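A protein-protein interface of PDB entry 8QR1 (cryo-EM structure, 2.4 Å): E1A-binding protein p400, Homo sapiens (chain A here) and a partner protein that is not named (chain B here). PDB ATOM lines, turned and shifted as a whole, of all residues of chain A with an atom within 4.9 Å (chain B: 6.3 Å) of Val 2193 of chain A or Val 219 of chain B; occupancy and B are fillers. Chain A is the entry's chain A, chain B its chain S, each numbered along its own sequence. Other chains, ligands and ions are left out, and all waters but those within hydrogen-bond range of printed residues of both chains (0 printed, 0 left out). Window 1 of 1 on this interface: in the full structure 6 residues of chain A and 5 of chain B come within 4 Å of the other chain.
The side-chain carboxylate of Glu 2197 of chain A lies within salt-bridge range of the guanidinium group of Arg 263 of chain B.
Among the printed residues, merely in contact across the chains: Val 2193 of chain A with Val 219 of chain B, Val 2193 of chain A with Pro 220 of chain B, Arg 2194 of chain A with Pro 220 of chain B, Trp 2196 of chain A with Arg 263 of chain B and Glu 2197 of chain A with Pro 220 of chain B.
Printed residues of chain B within 4 Å of Arg 2194 of chain A: Pro 220 (3.4 Å).
Printed residues of chain B within 4 Å of Trp 2196 of chain A: Arg 263 (3.5 Å).
Printed residues of chain B within 4 Å of Glu 2197 of chain A: Pro 220 and Arg 263.
Val 219 of chain B touches just one residue of chain A: Val 2193.
Printed residues of chain A within 4 Å of Pro 220 of chain B: Val 2193, Arg 2194 and Glu 2197.
The nearest residue of chain B that does not touch Val 2193 of chain A is Val 217 of chain B (5.2 Å).
The nearest printed residue of chain A that does not touch Arg 263 of chain B is Val 2193 of chain A (6.2 Å).
Of the 9 printed residues of chain A, 4 touch a printed residue of chain B.
Hydrophobic or aromatic side chains of chain A that line the printed part of chain B: Val 2193 and Trp 2196.
Of the 9 printed residues of chain B, 3 touch a printed residue of chain A.
Among the printed residues, 6 pairs touch across the chains.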
ATOM      1  N   VAL A2189      15.473  14.234 -31.825  1.00  0.00           N
ATOM      2  CA  VAL A2189      14.699  14.684 -30.672  1.00  0.00           C
ATOM      3  C   VAL A2189      13.367  13.940 -30.565  1.00  0.00           C
ATOM      4  O   VAL A2189      12.723  13.974 -29.508  1.00  0.00           O
ATOM      5  CB  VAL A2189      14.495  16.216 -30.761  1.00  0.00           C
ATOM      6  CG1 VAL A2189      13.739  16.744 -29.538  1.00  0.00           C
ATOM      7  CG2 VAL A2189      15.850  16.926 -30.927  1.00  0.00           C
ATOM      8  N   MET A2190      12.944  13.247 -31.633  1.00  0.00           N
ATOM      9  CA  MET A2190      11.685  12.508 -31.599  1.00  0.00           C
ATOM     10  C   MET A2190      11.695  11.413 -30.540  1.00  0.00           C
ATOM     11  O   MET A2190      10.644  11.089 -29.979  1.00  0.00           O
ATOM     12  CB  MET A2190      11.402  11.904 -32.974  1.00  0.00           C
ATOM     13  N   THR A2191      12.865  10.843 -30.241  1.00  0.00           N
ATOM     14  CA  THR A2191      12.960   9.892 -29.138  1.00  0.00           C
ATOM     15  C   THR A2191      12.630  10.561 -27.809  1.00  0.00           C
ATOM     16  O   THR A2191      11.899   9.996 -26.983  1.00  0.00           O
ATOM     17  CB  THR A2191      14.362   9.282 -29.088  1.00  0.00           C
ATOM     18  OG1 THR A2191      15.327  10.316 -28.860  1.00  0.00           O
ATOM     19  CG2 THR A2191      14.686   8.564 -30.390  1.00  0.00           C
ATOM     20  N   ALA A2192      13.155  11.770 -27.592  1.00  0.00           N
ATOM     21  CA  ALA A2192      12.846  12.506 -26.373  1.00  0.00           C
ATOM     22  C   ALA A2192      11.368  12.858 -26.303  1.00  0.00           C
ATOM     23  O   ALA A2192      10.760  12.796 -25.229  1.00  0.00           O
ATOM     24  CB  ALA A2192      13.698  13.771 -26.293  1.00  0.00           C
ATOM     25  N   VAL A2193      10.773  13.229 -27.438  1.00  0.00           N
ATOM     26  CA  VAL A2193       9.348  13.555 -27.450  1.00  0.00           C
ATOM     27  C   VAL A2193       8.517  12.316 -27.139  1.00  0.00           C
ATOM     28  O   VAL A2193       7.516  12.391 -26.418  1.00  0.00           O
ATOM     29  CB  VAL A2193       8.936  14.180 -28.796  1.00  0.00           C
ATOM     30  CG1 VAL A2193       7.439  14.449 -28.801  1.00  0.00           C
ATOM     31  CG2 VAL A2193       9.690  15.478 -29.066  1.00  0.00           C
ATOM     32  N   ARG A2194       8.908  11.162 -27.689  1.00  0.00           N
ATOM     33  CA  ARG A2194       8.213   9.909 -27.399  1.00  0.00           C
ATOM     34  C   ARG A2194       8.284   9.580 -25.915  1.00  0.00           C
ATOM     35  O   ARG A2194       7.275   9.218 -25.294  1.00  0.00           O
ATOM     36  CB  ARG A2194       8.826   8.772 -28.217  1.00  0.00           C
ATOM     37  CG  ARG A2194       8.278   8.626 -29.628  1.00  0.00           C
ATOM     38  CD  ARG A2194       6.939   7.905 -29.662  1.00  0.00           C
ATOM     39  NE  ARG A2194       6.575   7.508 -31.017  1.00  0.00           N
ATOM     40  CZ  ARG A2194       5.538   6.743 -31.341  1.00  0.00           C
ATOM     41  NH1 ARG A2194       4.710   6.259 -30.426  1.00  0.00           N
ATOM     42  NH2 ARG A2194       5.323   6.455 -32.621  1.00  0.00           N
ATOM     43  N   ALA A2195       9.480   9.708 -25.332  1.00  0.00           N
ATOM     44  CA  ALA A2195       9.650   9.426 -23.911  1.00  0.00           C
ATOM     45  C   ALA A2195       8.822  10.377 -23.060  1.00  0.00           C
ATOM     46  O   ALA A2195       8.193   9.960 -22.079  1.00  0.00           O
ATOM     47  CB  ALA A2195      11.127   9.523 -23.536  1.00  0.00           C
ATOM     48  N   TRP A2196       8.798  11.660 -23.431  1.00  0.00           N
ATOM     49  CA  TRP A2196       7.995  12.627 -22.694  1.00  0.00           C
ATOM     50  C   TRP A2196       6.514  12.302 -22.795  1.00  0.00           C
ATOM     51  O   TRP A2196       5.775  12.457 -21.820  1.00  0.00           O
ATOM     52  CB  TRP A2196       8.253  14.042 -23.207  1.00  0.00           C
ATOM     53  CG  TRP A2196       7.572  15.097 -22.387  1.00  0.00           C
ATOM     54  CD1 TRP A2196       8.098  15.770 -21.329  1.00  0.00           C
ATOM     55  CD2 TRP A2196       6.237  15.595 -22.552  1.00  0.00           C
ATOM     56  NE1 TRP A2196       7.182  16.657 -20.826  1.00  0.00           N
ATOM     57  CE2 TRP A2196       6.029  16.566 -21.558  1.00  0.00           C
ATOM     58  CE3 TRP A2196       5.198  15.308 -23.442  1.00  0.00           C
ATOM     59  CZ2 TRP A2196       4.830  17.257 -21.429  1.00  0.00           C
ATOM     60  CZ3 TRP A2196       4.008  15.993 -23.311  1.00  0.00           C
ATOM     61  CH2 TRP A2196       3.833  16.956 -22.313  1.00  0.00           C
ATOM     62  N   GLU A2197       6.052  11.889 -23.976  1.00  0.00           N
ATOM     63  CA  GLU A2197       4.636  11.580 -24.131  1.00  0.00           C
ATOM     64  C   GLU A2197       4.245  10.364 -23.304  1.00  0.00           C
ATOM     65  O   GLU A2197       3.179  10.355 -22.677  1.00  0.00           O
ATOM     66  CB  GLU A2197       4.293  11.356 -25.604  1.00  0.00           C
ATOM     67  CG  GLU A2197       4.046  12.629 -26.414  1.00  0.00           C
ATOM     68  CD  GLU A2197       2.889  12.492 -27.385  1.00  0.00           C
ATOM     69  OE1 GLU A2197       2.748  11.417 -28.004  1.00  0.00           O
ATOM     70  OE2 GLU A2197       2.116  13.462 -27.528  1.00  0.00           O
ATOM     71  N   VAL B 217       4.860  21.315 -31.905  1.00  0.00           N
ATOM     72  CA  VAL B 217       5.804  20.382 -32.527  1.00  0.00           C
ATOM     73  C   VAL B 217       5.133  19.211 -33.243  1.00  0.00           C
ATOM     74  O   VAL B 217       5.700  18.650 -34.187  1.00  0.00           O
ATOM     75  CB  VAL B 217       6.799  19.865 -31.468  1.00  0.00           C
ATOM     76  CG1 VAL B 217       7.709  20.989 -31.012  1.00  0.00           C
ATOM     77  CG2 VAL B 217       6.071  19.280 -30.254  1.00  0.00           C
ATOM     78  N   THR B 218       3.935  18.819 -32.798  1.00  0.00           N
ATOM     79  CA  THR B 218       3.164  17.707 -33.369  1.00  0.00           C
ATOM     80  C   THR B 218       3.760  16.309 -33.225  1.00  0.00           C
ATOM     81  O   THR B 218       3.110  15.337 -33.622  1.00  0.00           O
ATOM     82  CB  THR B 218       2.885  17.901 -34.868  1.00  0.00           C
ATOM     83  OG1 THR B 218       4.002  17.434 -35.636  1.00  0.00           O
ATOM     84  CG2 THR B 218       2.524  19.319 -35.217  1.00  0.00           C
ATOM     85  N   VAL B 219       4.960  16.169 -32.671  1.00  0.00           N
ATOM     86  CA  VAL B 219       5.593  14.847 -32.729  1.00  0.00           C
ATOM     87  C   VAL B 219       4.934  13.943 -31.689  1.00  0.00           C
ATOM     88  O   VAL B 219       4.617  14.418 -30.579  1.00  0.00           O
ATOM     89  CB  VAL B 219       7.110  14.956 -32.495  1.00  0.00           C
ATOM     90  CG1 VAL B 219       7.738  13.572 -32.296  1.00  0.00           C
ATOM     91  CG2 VAL B 219       7.776  15.681 -33.661  1.00  0.00           C
ATOM     92  N   PRO B 220       4.677  12.648 -31.974  1.00  0.00           N
ATOM     93  CA  PRO B 220       4.152  11.822 -30.880  1.00  0.00           C
ATOM     94  C   PRO B 220       5.178  11.580 -29.781  1.00  0.00           C
ATOM     95  O   PRO B 220       6.338  11.331 -30.105  1.00  0.00           O
ATOM     96  CB  PRO B 220       3.790  10.505 -31.570  1.00  0.00           C
ATOM     97  CG  PRO B 220       3.630  10.834 -32.987  1.00  0.00           C
ATOM     98  CD  PRO B 220       4.598  11.936 -33.263  1.00  0.00           C
ATOM     99  N   ALA B 259       0.308   8.565 -31.240  1.00  0.00           N
ATOM    100  CA  ALA B 259      -0.559   9.140 -32.260  1.00  0.00           C
ATOM    101  C   ALA B 259      -0.051  10.511 -32.681  1.00  0.00           C
ATOM    102  O   ALA B 259       0.516  11.242 -31.868  1.00  0.00           O
ATOM    103  CB  ALA B 259      -1.986   9.243 -31.744  1.00  0.00           C
ATOM    104  N   ARG B 260      -0.244  10.853 -33.953  1.00  0.00           N
ATOM    105  CA  ARG B 260       0.089  12.192 -34.419  1.00  0.00           C
ATOM    106  C   ARG B 260      -0.799  13.209 -33.716  1.00  0.00           C
ATOM    107  O   ARG B 260      -2.016  13.029 -33.614  1.00  0.00           O
ATOM    108  CB  ARG B 260      -0.079  12.302 -35.933  1.00  0.00           C
ATOM    109  CG  ARG B 260       1.074  11.714 -36.760  1.00  0.00           C
ATOM    110  CD  ARG B 260       1.180  10.189 -36.686  1.00  0.00           C
ATOM    111  NE  ARG B 260      -0.078   9.523 -37.018  1.00  0.00           N
ATOM    112  CZ  ARG B 260      -0.460   8.321 -36.602  1.00  0.00           C
ATOM    113  NH1 ARG B 260       0.312   7.561 -35.837  1.00  0.00           N
ATOM    114  NH2 ARG B 260      -1.651   7.860 -36.969  1.00  0.00           N
ATOM    115  N   CYS B 261      -0.180  14.287 -33.242  1.00  0.00           N
ATOM    116  CA  CYS B 261      -0.774  15.155 -32.235  1.00  0.00           C
ATOM    117  C   CYS B 261      -0.434  16.605 -32.558  1.00  0.00           C
ATOM    118  O   CYS B 261       0.038  16.930 -33.651  1.00  0.00           O
ATOM    119  CB  CYS B 261      -0.271  14.742 -30.847  1.00  0.00           C
ATOM    120  SG  CYS B 261      -1.265  15.334 -29.487  1.00  0.00           S
ATOM    121  N   SER B 262      -0.713  17.481 -31.595  1.00  0.00           N
ATOM    122  CA  SER B 262      -0.309  18.877 -31.641  1.00  0.00           C
ATOM    123  C   SER B 262      -0.410  19.434 -30.231  1.00  0.00           C
ATOM    124  O   SER B 262      -1.424  19.238 -29.557  1.00  0.00           O
ATOM    125  CB  SER B 262      -1.172  19.696 -32.607  1.00  0.00           C
ATOM    126  OG  SER B 262      -2.538  19.357 -32.499  1.00  0.00           O
ATOM    127  N   ARG B 263       0.644  20.128 -29.801  1.00  0.00           N
ATOM    128  CA  ARG B 263       0.794  20.577 -28.424  1.00  0.00           C
ATOM    129  C   ARG B 263       1.220  22.035 -28.400  1.00  0.00           C
ATOM    130  O   ARG B 263       1.508  22.642 -29.434  1.00  0.00           O
ATOM    131  CB  ARG B 263       1.828  19.734 -27.678  1.00  0.00           C
ATOM    132  CG  ARG B 263       1.659  18.245 -27.857  1.00  0.00           C
ATOM    133  CD  ARG B 263       2.455  17.483 -26.817  1.00  0.00           C
ATOM    134  NE  ARG B 263       1.825  17.553 -25.500  1.00  0.00           N
ATOM    135  CZ  ARG B 263       0.900  16.722 -25.035  1.00  0.00           C
ATOM    136  NH1 ARG B 263       0.440  15.706 -25.751  1.00  0.00           N
ATOM    137  NH2 ARG B 263       0.410  16.920 -23.816  1.00  0.00           N
